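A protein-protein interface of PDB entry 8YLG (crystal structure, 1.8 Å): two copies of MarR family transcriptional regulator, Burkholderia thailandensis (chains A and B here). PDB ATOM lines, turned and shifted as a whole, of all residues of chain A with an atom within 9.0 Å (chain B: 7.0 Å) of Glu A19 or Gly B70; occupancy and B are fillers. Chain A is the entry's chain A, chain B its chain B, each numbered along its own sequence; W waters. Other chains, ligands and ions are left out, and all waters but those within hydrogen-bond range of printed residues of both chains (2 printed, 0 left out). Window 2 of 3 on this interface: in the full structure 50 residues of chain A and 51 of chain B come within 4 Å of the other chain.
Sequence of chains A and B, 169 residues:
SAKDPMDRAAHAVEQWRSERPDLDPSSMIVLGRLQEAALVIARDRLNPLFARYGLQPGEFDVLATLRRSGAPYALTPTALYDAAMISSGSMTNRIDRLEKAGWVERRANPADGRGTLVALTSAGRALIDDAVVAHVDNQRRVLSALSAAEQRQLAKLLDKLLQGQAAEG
Of chain B, only Arg B67, Arg B68 and Gly B70 come within 4 Å of Glu A19.
Of chain A, only Gln A15 (3.96 Å) comes within 4 Å of Ser B69.
No residue of chain A comes within 4 Å of Ala B71.
Of the printed residues of chain B, Gln A15 touches Arg B68 and Ser B69.
Of the printed residues of chain B, Ala A12 touches Arg B68.
Of the printed residues of chain A, Arg B67 touches Trp A16, Glu A19 and Arg A20.
Of the printed residues of chain A, Asp B129 touches Arg A20 (3.0 Å).
Printed residues of chain B within 4 Å of Arg A20: Arg B67 (3.4 Å) and Asp B129 (3.0 Å).
Tyr B73 touches none of the printed residues of chain A.
Leu A23 touches none of the printed residues of chain B.
The nearest residue of chain B that does not touch Glu A19 is Tyr B73 (4.1 Å).
The nearest printed residue of chain B that does not touch Trp A16 is Asp B129 (5.2 Å).
Water W1 lies within hydrogen-bond range of the backbone carbonyl oxygen of Thr B65 (3.0 Å) and the side-chain amide nitrogen of Gln A15 (3.1 Å).
Water W2 lies within hydrogen-bond range of the guanidinium group of Arg A20 (3.0 Å) and the backbone carbonyl oxygen of Asp B129 (3.1 Å).
The backbone carbonyl oxygen of Leu B66 lies within hydrogen-bond range of the side-chain hydroxyl of Ser B69 (2.7 Å).
The guanidinium group (NH2) of Arg A20 lies within salt-bridge range of the side-chain carboxylate (OD2) of Asp A22 (2.8 Å).
The guanidinium group (NE) of Arg B67 is in salt-bridge range of the side-chain carboxylate (OD1) of Asp B129, 2.8 Å away.
The guanidinium group (NE) of Arg B125 lies within salt-bridge range of the side-chain carboxylate (OD2) of Asp B129 (2.8 Å).
Among the printed residues, pairs that only touch across the chains: Glu A19 with Gly B70, Arg A20 with Arg B67, Glu A19 with Arg B68, Trp A16 with Arg B67, Trp A16 with Arg B68, Ala A12 with Arg B68 and Gln A15 with Ser B69.
No position is printed for both chains.
The guanidinium group (NH1) of Arg A20 is in salt-bridge range of the side-chain carboxylate (OD1) of Asp B129 (3.1 Å).
The side-chain amide oxygen of Gln A15 lies within hydrogen-bond range of the guanidinium group of Arg B68, at 2.8 Å.
The guanidinium group (NH1) of Arg B67 is in salt-bridge range of the side-chain carboxylate (OE1) of Glu A19.
Of the 13 printed residues of chain A, 5 touch a printed residue of chain B.
Along chain B the printed residues that touch a printed residue of chain A span positions 67 to 129.
Among the printed residues, Asp or Glu carboxylates within 4 Å of a Lys or Arg side-chain nitrogen of the other chain: Glu A19 with Arg B67 (2.8 Å) and Arg A20 with Asp B129 (3.1 Å).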
ATOM      1  N   ALA A  12      -9.304  22.466 -17.506  1.00  0.00           N
ATOM      2  CA  ALA A  12      -9.912  23.185 -18.624  1.00  0.00           C
ATOM      3  C   ALA A  12     -10.253  22.239 -19.766  1.00  0.00           C
ATOM      4  O   ALA A  12     -11.313  22.363 -20.387  1.00  0.00           O
ATOM      5  CB  ALA A  12      -8.986  24.300 -19.106  1.00  0.00           C
ATOM      6  N   VAL A  13      -9.372  21.278 -20.054  1.00  0.00           N
ATOM      7  CA  VAL A  13      -9.663  20.310 -21.113  1.00  0.00           C
ATOM      8  C   VAL A  13     -10.861  19.440 -20.752  1.00  0.00           C
ATOM      9  O   VAL A  13     -11.711  19.151 -21.600  1.00  0.00           O
ATOM     10  CB  VAL A  13      -8.409  19.473 -21.420  1.00  0.00           C
ATOM     11  CG1 VAL A  13      -8.772  18.186 -22.144  1.00  0.00           C
ATOM     12  CG2 VAL A  13      -7.462  20.313 -22.257  1.00  0.00           C
ATOM     13  N   GLU A  14     -10.952  19.002 -19.493  1.00  0.00           N
ATOM     14  CA  GLU A  14     -12.118  18.234 -19.070  1.00  0.00           C
ATOM     15  C   GLU A  14     -13.403  19.034 -19.246  1.00  0.00           C
ATOM     16  O   GLU A  14     -14.439  18.484 -19.639  1.00  0.00           O
ATOM     17  CB  GLU A  14     -11.956  17.786 -17.617  1.00  0.00           C
ATOM     18  CG  GLU A  14     -10.942  16.674 -17.453  1.00  0.00           C
ATOM     19  CD  GLU A  14     -11.151  15.551 -18.461  1.00  0.00           C
ATOM     20  OE1 GLU A  14     -12.266  14.979 -18.498  1.00  0.00           O
ATOM     21  OE2 GLU A  14     -10.205  15.257 -19.229  1.00  0.00           O
ATOM     22  N   GLN A  15     -13.367  20.332 -18.933  1.00  0.00           N
ATOM     23  CA  GLN A  15     -14.548  21.161 -19.145  1.00  0.00           C
ATOM     24  C   GLN A  15     -14.925  21.207 -20.622  1.00  0.00           C
ATOM     25  O   GLN A  15     -16.095  21.031 -20.982  1.00  0.00           O
ATOM     26  CB  GLN A  15     -14.303  22.565 -18.601  1.00  0.00           C
ATOM     27  CG  GLN A  15     -14.162  22.635 -17.093  1.00  0.00           C
ATOM     28  CD  GLN A  15     -13.864  24.038 -16.638  1.00  0.00           C
ATOM     29  OE1 GLN A  15     -12.840  24.624 -17.012  1.00  0.00           O
ATOM     30  NE2 GLN A  15     -14.770  24.605 -15.856  1.00  0.00           N
ATOM     31  N   TRP A  16     -13.932  21.422 -21.500  1.00  0.00           N
ATOM     32  CA  TRP A  16     -14.217  21.483 -22.937  1.00  0.00           C
ATOM     33  C   TRP A  16     -14.720  20.148 -23.467  1.00  0.00           C
ATOM     34  O   TRP A  16     -15.619  20.114 -24.318  1.00  0.00           O
ATOM     35  CB  TRP A  16     -12.969  21.915 -23.710  1.00  0.00           C
ATOM     36  CG  TRP A  16     -12.739  23.376 -23.704  1.00  0.00           C
ATOM     37  CD1 TRP A  16     -11.653  24.035 -23.195  1.00  0.00           C
ATOM     38  CD2 TRP A  16     -13.597  24.381 -24.252  1.00  0.00           C
ATOM     39  NE1 TRP A  16     -11.788  25.390 -23.390  1.00  0.00           N
ATOM     40  CE2 TRP A  16     -12.972  25.628 -24.037  1.00  0.00           C
ATOM     41  CE3 TRP A  16     -14.837  24.346 -24.905  1.00  0.00           C
ATOM     42  CZ2 TRP A  16     -13.546  26.833 -24.446  1.00  0.00           C
ATOM     43  CZ3 TRP A  16     -15.403  25.545 -25.311  1.00  0.00           C
ATOM     44  CH2 TRP A  16     -14.759  26.768 -25.083  1.00  0.00           C
ATOM     45  N   ARG A  17     -14.150  19.033 -22.992  1.00  0.00           N
ATOM     46  CA  ARG A  17     -14.646  17.726 -23.426  1.00  0.00           C
ATOM     47  C   ARG A  17     -16.118  17.568 -23.079  1.00  0.00           C
ATOM     48  O   ARG A  17     -16.883  16.941 -23.822  1.00  0.00           O
ATOM     49  CB  ARG A  17     -13.846  16.592 -22.781  1.00  0.00           C
ATOM     50  CG  ARG A  17     -12.403  16.438 -23.254  1.00  0.00           C
ATOM     51  CD  ARG A  17     -11.842  15.112 -22.739  1.00  0.00           C
ATOM     52  NE  ARG A  17     -10.380  15.065 -22.698  1.00  0.00           N
ATOM     53  CZ  ARG A  17      -9.594  14.912 -23.761  1.00  0.00           C
ATOM     54  NH1 ARG A  17     -10.118  14.803 -24.979  1.00  0.00           N
ATOM     55  NH2 ARG A  17      -8.276  14.878 -23.604  1.00  0.00           N
ATOM     56  N   SER A  18     -16.529  18.120 -21.941  1.00  0.00           N
ATOM     57  CA  SER A  18     -17.929  18.036 -21.546  1.00  0.00           C
ATOM     58  C   SER A  18     -18.800  18.984 -22.364  1.00  0.00           C
ATOM     59  O   SER A  18     -19.883  18.602 -22.819  1.00  0.00           O
ATOM     60  CB  SER A  18     -18.062  18.343 -20.054  1.00  0.00           C
ATOM     61  OG  SER A  18     -19.426  18.520 -19.712  1.00  0.00           O
ATOM     62  N   GLU A  19     -18.341  20.225 -22.554  1.00  0.00           N
ATOM     63  CA  GLU A  19     -19.150  21.288 -23.149  1.00  0.00           C
ATOM     64  C   GLU A  19     -19.154  21.273 -24.671  1.00  0.00           C
ATOM     65  O   GLU A  19     -20.115  21.748 -25.279  1.00  0.00           O
ATOM     66  CB  GLU A  19     -18.661  22.652 -22.659  1.00  0.00           C
ATOM     67  CG  GLU A  19     -19.121  22.959 -21.244  1.00  0.00           C
ATOM     68  CD  GLU A  19     -20.639  23.054 -21.168  1.00  0.00           C
ATOM     69  OE1 GLU A  19     -21.234  23.704 -22.056  1.00  0.00           O
ATOM     70  OE2 GLU A  19     -21.240  22.457 -20.251  1.00  0.00           O
ATOM     71  N   ARG A  20     -18.094  20.788 -25.303  1.00  0.00           N
ATOM     72  CA  ARG A  20     -17.997  20.741 -26.764  1.00  0.00           C
ATOM     73  C   ARG A  20     -17.477  19.363 -27.134  1.00  0.00           C
ATOM     74  O   ARG A  20     -16.314  19.206 -27.524  1.00  0.00           O
ATOM     75  CB  ARG A  20     -17.092  21.852 -27.308  1.00  0.00           C
ATOM     76  CG  ARG A  20     -17.643  23.273 -27.131  1.00  0.00           C
ATOM     77  CD  ARG A  20     -18.809  23.566 -28.101  1.00  0.00           C
ATOM     78  NE  ARG A  20     -18.461  23.261 -29.489  1.00  0.00           N
ATOM     79  CZ  ARG A  20     -18.080  24.166 -30.385  1.00  0.00           C
ATOM     80  NH1 ARG A  20     -18.009  25.450 -30.053  1.00  0.00           N
ATOM     81  NH2 ARG A  20     -17.775  23.785 -31.621  1.00  0.00           N
ATOM     82  N   PRO A  21     -18.322  18.330 -27.040  1.00  0.00           N
ATOM     83  CA  PRO A  21     -17.863  16.981 -27.397  1.00  0.00           C
ATOM     84  C   PRO A  21     -17.528  16.840 -28.874  1.00  0.00           C
ATOM     85  O   PRO A  21     -16.906  15.843 -29.262  1.00  0.00           O
ATOM     86  CB  PRO A  21     -19.042  16.087 -26.990  1.00  0.00           C
ATOM     87  CG  PRO A  21     -20.237  16.990 -27.016  1.00  0.00           C
ATOM     88  CD  PRO A  21     -19.728  18.350 -26.607  1.00  0.00           C
ATOM     89  N   ASP A  22     -17.914  17.803 -29.708  1.00  0.00           N
ATOM     90  CA  ASP A  22     -17.531  17.765 -31.111  1.00  0.00           C
ATOM     91  C   ASP A  22     -16.066  18.144 -31.327  1.00  0.00           C
ATOM     92  O   ASP A  22     -15.552  17.961 -32.435  1.00  0.00           O
ATOM     93  CB  ASP A  22     -18.436  18.703 -31.908  1.00  0.00           C
ATOM     94  CG  ASP A  22     -18.366  20.137 -31.408  1.00  0.00           C
ATOM     95  OD1 ASP A  22     -18.620  20.365 -30.200  1.00  0.00           O
ATOM     96  OD2 ASP A  22     -18.026  21.034 -32.213  1.00  0.00           O
ATOM     97  N   LEU A  23     -15.380  18.607 -30.292  1.00  0.00           N
ATOM     98  CA  LEU A  23     -14.015  19.117 -30.388  1.00  0.00           C
ATOM     99  C   LEU A  23     -13.048  18.206 -29.649  1.00  0.00           C
ATOM    100  O   LEU A  23     -13.391  17.645 -28.606  1.00  0.00           O
ATOM    101  CB  LEU A  23     -13.900  20.514 -29.783  1.00  0.00           C
ATOM    102  CG  LEU A  23     -14.427  21.710 -30.560  1.00  0.00           C
ATOM    103  CD1 LEU A  23     -13.757  22.971 -30.036  1.00  0.00           C
ATOM    104  CD2 LEU A  23     -14.177  21.528 -32.055  1.00  0.00           C
ATOM    105  N   PRO A  25      -9.916  18.866 -27.665  1.00  0.00           N
ATOM    106  CA  PRO A  25      -9.123  19.999 -27.171  1.00  0.00           C
ATOM    107  C   PRO A  25      -7.817  19.583 -26.508  1.00  0.00           C
ATOM    108  O   PRO A  25      -7.227  20.366 -25.762  1.00  0.00           O
ATOM    109  CB  PRO A  25     -10.073  20.638 -26.157  1.00  0.00           C
ATOM    110  CG  PRO A  25     -10.746  19.433 -25.532  1.00  0.00           C
ATOM    111  CD  PRO A  25     -10.809  18.344 -26.617  1.00  0.00           C
ATOM    112  N   THR B  65     -13.063  30.746 -20.771  1.00  0.00           N
ATOM    113  CA  THR B  65     -13.328  30.307 -19.401  1.00  0.00           C
ATOM    114  C   THR B  65     -14.822  30.323 -19.103  1.00  0.00           C
ATOM    115  O   THR B  65     -15.356  29.392 -18.491  1.00  0.00           O
ATOM    116  CB  THR B  65     -12.573  31.212 -18.418  1.00  0.00           C
ATOM    117  OG1 THR B  65     -11.172  31.242 -18.751  1.00  0.00           O
ATOM    118  CG2 THR B  65     -12.750  30.734 -16.959  1.00  0.00           C
ATOM    119  N   LEU B  66     -15.515  31.377 -19.528  1.00  0.00           N
ATOM    120  CA  LEU B  66     -16.970  31.412 -19.368  1.00  0.00           C
ATOM    121  C   LEU B  66     -17.650  30.278 -20.127  1.00  0.00           C
ATOM    122  O   LEU B  66     -18.522  29.587 -19.585  1.00  0.00           O
ATOM    123  CB  LEU B  66     -17.502  32.768 -19.840  1.00  0.00           C
ATOM    124  CG  LEU B  66     -17.113  33.963 -18.967  1.00  0.00           C
ATOM    125  CD1 LEU B  66     -17.479  35.272 -19.664  1.00  0.00           C
ATOM    126  CD2 LEU B  66     -17.778  33.862 -17.580  1.00  0.00           C
ATOM    127  N   ARG B  67     -17.275  30.076 -21.394  1.00  0.00           N
ATOM    128  CA  ARG B  67     -17.960  29.079 -22.216  1.00  0.00           C
ATOM    129  C   ARG B  67     -17.752  27.673 -21.664  1.00  0.00           C
ATOM    130  O   ARG B  67     -18.699  26.883 -21.555  1.00  0.00           O
ATOM    131  CB  ARG B  67     -17.472  29.175 -23.673  1.00  0.00           C
ATOM    132  CG  ARG B  67     -18.015  28.067 -24.588  1.00  0.00           C
ATOM    133  CD  ARG B  67     -19.533  28.213 -24.800  1.00  0.00           C
ATOM    134  NE  ARG B  67     -20.093  27.087 -25.554  1.00  0.00           N
ATOM    135  CZ  ARG B  67     -20.435  25.918 -25.018  1.00  0.00           C
ATOM    136  NH1 ARG B  67     -20.280  25.705 -23.716  1.00  0.00           N
ATOM    137  NH2 ARG B  67     -20.940  24.955 -25.782  1.00  0.00           N
ATOM    138  N   ARG B  68     -16.514  27.341 -21.300  1.00  0.00           N
ATOM    139  CA  ARG B  68     -16.241  25.984 -20.852  1.00  0.00           C
ATOM    140  C   ARG B  68     -16.834  25.688 -19.478  1.00  0.00           C
ATOM    141  O   ARG B  68     -16.909  24.518 -19.102  1.00  0.00           O
ATOM    142  CB  ARG B  68     -14.727  25.725 -20.850  1.00  0.00           C
ATOM    143  CG  ARG B  68     -13.974  26.465 -19.784  1.00  0.00           C
ATOM    144  CD  ARG B  68     -12.462  26.218 -19.896  1.00  0.00           C
ATOM    145  NE  ARG B  68     -11.771  26.650 -18.682  1.00  0.00           N
ATOM    146  CZ  ARG B  68     -10.726  27.472 -18.641  1.00  0.00           C
ATOM    147  NH1 ARG B  68     -10.203  27.956 -19.762  1.00  0.00           N
ATOM    148  NH2 ARG B  68     -10.196  27.797 -17.469  1.00  0.00           N
ATOM    149  N   SER B  69     -17.254  26.707 -18.725  1.00  0.00           N
ATOM    150  CA  SER B  69     -17.881  26.476 -17.430  1.00  0.00           C
ATOM    151  C   SER B  69     -19.330  26.011 -17.546  1.00  0.00           C
ATOM    152  O   SER B  69     -19.905  25.571 -16.540  1.00  0.00           O
ATOM    153  CB  SER B  69     -17.816  27.744 -16.579  1.00  0.00           C
ATOM    154  OG  SER B  69     -18.718  28.722 -17.066  1.00  0.00           O
ATOM    155  N   GLY B  70     -19.928  26.085 -18.736  1.00  0.00           N
ATOM    156  CA  GLY B  70     -21.278  25.600 -18.953  1.00  0.00           C
ATOM    157  C   GLY B  70     -22.332  26.645 -18.635  1.00  0.00           C
ATOM    158  O   GLY B  70     -22.073  27.683 -18.017  1.00  0.00           O
ATOM    159  N   ALA B  71     -23.553  26.362 -19.088  1.00  0.00           N
ATOM    160  CA  ALA B  71     -24.653  27.292 -18.886  1.00  0.00           C
ATOM    161  C   ALA B  71     -24.839  27.567 -17.393  1.00  0.00           C
ATOM    162  O   ALA B  71     -24.715  26.651 -16.575  1.00  0.00           O
ATOM    163  CB  ALA B  71     -25.945  26.725 -19.481  1.00  0.00           C
ATOM    164  N   PRO B  72     -25.162  28.808 -17.002  1.00  0.00           N
ATOM    165  CA  PRO B  72     -25.427  29.932 -17.905  1.00  0.00           C
ATOM    166  C   PRO B  72     -24.205  30.771 -18.247  1.00  0.00           C
ATOM    167  O   PRO B  72     -24.379  31.958 -18.504  1.00  0.00           O
ATOM    168  CB  PRO B  72     -26.430  30.765 -17.112  1.00  0.00           C
ATOM    169  CG  PRO B  72     -26.022  30.553 -15.690  1.00  0.00           C
ATOM    170  CD  PRO B  72     -25.421  29.164 -15.599  1.00  0.00           C
ATOM    171  N   TYR B  73     -23.016  30.162 -18.270  1.00  0.00           N
ATOM    172  CA  TYR B  73     -21.781  30.831 -18.695  1.00  0.00           C
ATOM    173  C   TYR B  73     -21.565  32.135 -17.935  1.00  0.00           C
ATOM    174  O   TYR B  73     -21.290  33.193 -18.517  1.00  0.00           O
ATOM    175  CB  TYR B  73     -21.782  31.071 -20.210  1.00  0.00           C
ATOM    176  CG  TYR B  73     -22.408  29.937 -20.979  1.00  0.00           C
ATOM    177  CD1 TYR B  73     -21.733  28.740 -21.160  1.00  0.00           C
ATOM    178  CD2 TYR B  73     -23.681  30.059 -21.511  1.00  0.00           C
ATOM    179  CE1 TYR B  73     -22.308  27.690 -21.859  1.00  0.00           C
ATOM    180  CE2 TYR B  73     -24.271  29.011 -22.209  1.00  0.00           C
ATOM    181  CZ  TYR B  73     -23.576  27.830 -22.379  1.00  0.00           C
ATOM    182  OH  TYR B  73     -24.148  26.782 -23.071  1.00  0.00           O
ATOM    183  N   ALA B  74     -21.658  32.049 -16.607  1.00  0.00           N
ATOM    184  CA  ALA B  74     -21.549  33.219 -15.741  1.00  0.00           C
ATOM    185  C   ALA B  74     -20.603  32.903 -14.597  1.00  0.00           C
ATOM    186  O   ALA B  74     -20.832  31.943 -13.849  1.00  0.00           O
ATOM    187  CB  ALA B  74     -22.923  33.641 -15.201  1.00  0.00           C
ATOM    188  N   LEU B  75     -19.555  33.721 -14.454  1.00  0.00           N
ATOM    189  CA  LEU B  75     -18.543  33.535 -13.427  1.00  0.00           C
ATOM    190  C   LEU B  75     -18.231  34.872 -12.763  1.00  0.00           C
ATOM    191  O   LEU B  75     -18.366  35.941 -13.370  1.00  0.00           O
ATOM    192  CB  LEU B  75     -17.259  32.940 -14.029  1.00  0.00           C
ATOM    193  CG  LEU B  75     -17.399  31.532 -14.623  1.00  0.00           C
ATOM    194  CD1 LEU B  75     -16.121  31.159 -15.352  1.00  0.00           C
ATOM    195  CD2 LEU B  75     -17.724  30.515 -13.540  1.00  0.00           C
ATOM    196  N   ARG B 125     -21.165  34.216 -26.929  1.00  0.00           N
ATOM    197  CA  ARG B 125     -21.132  32.756 -27.043  1.00  0.00           C
ATOM    198  C   ARG B 125     -20.901  32.325 -28.488  1.00  0.00           C
ATOM    199  O   ARG B 125     -20.080  31.439 -28.758  1.00  0.00           O
ATOM    200  CB  ARG B 125     -22.435  32.150 -26.496  1.00  0.00           C
ATOM    201  CG  ARG B 125     -22.457  30.610 -26.326  1.00  0.00           C
ATOM    202  CD  ARG B 125     -23.337  29.925 -27.382  1.00  0.00           C
ATOM    203  NE  ARG B 125     -23.414  28.455 -27.291  1.00  0.00           N
ATOM    204  CZ  ARG B 125     -24.388  27.757 -26.696  1.00  0.00           C
ATOM    205  NH1 ARG B 125     -25.416  28.366 -26.112  1.00  0.00           N
ATOM    206  NH2 ARG B 125     -24.350  26.429 -26.712  1.00  0.00           N
ATOM    207  N   ASP B 129     -17.622  30.253 -29.562  1.00  0.00           N
ATOM    208  CA  ASP B 129     -17.881  28.923 -30.106  1.00  0.00           C
ATOM    209  C   ASP B 129     -17.201  28.715 -31.454  1.00  0.00           C
ATOM    210  O   ASP B 129     -16.816  27.586 -31.786  1.00  0.00           O
ATOM    211  CB  ASP B 129     -19.379  28.686 -30.256  1.00  0.00           C
ATOM    212  CG  ASP B 129     -20.002  28.068 -29.026  1.00  0.00           C
ATOM    213  OD1 ASP B 129     -19.261  27.580 -28.146  1.00  0.00           O
ATOM    214  OD2 ASP B 129     -21.252  28.028 -28.967  1.00  0.00           O
HETATM  215  O   HOH W   1     -14.276  27.600 -16.382  1.00  0.00           O
HETATM  216  O   HOH W   2     -18.441  25.866 -33.718  1.00  0.00           O
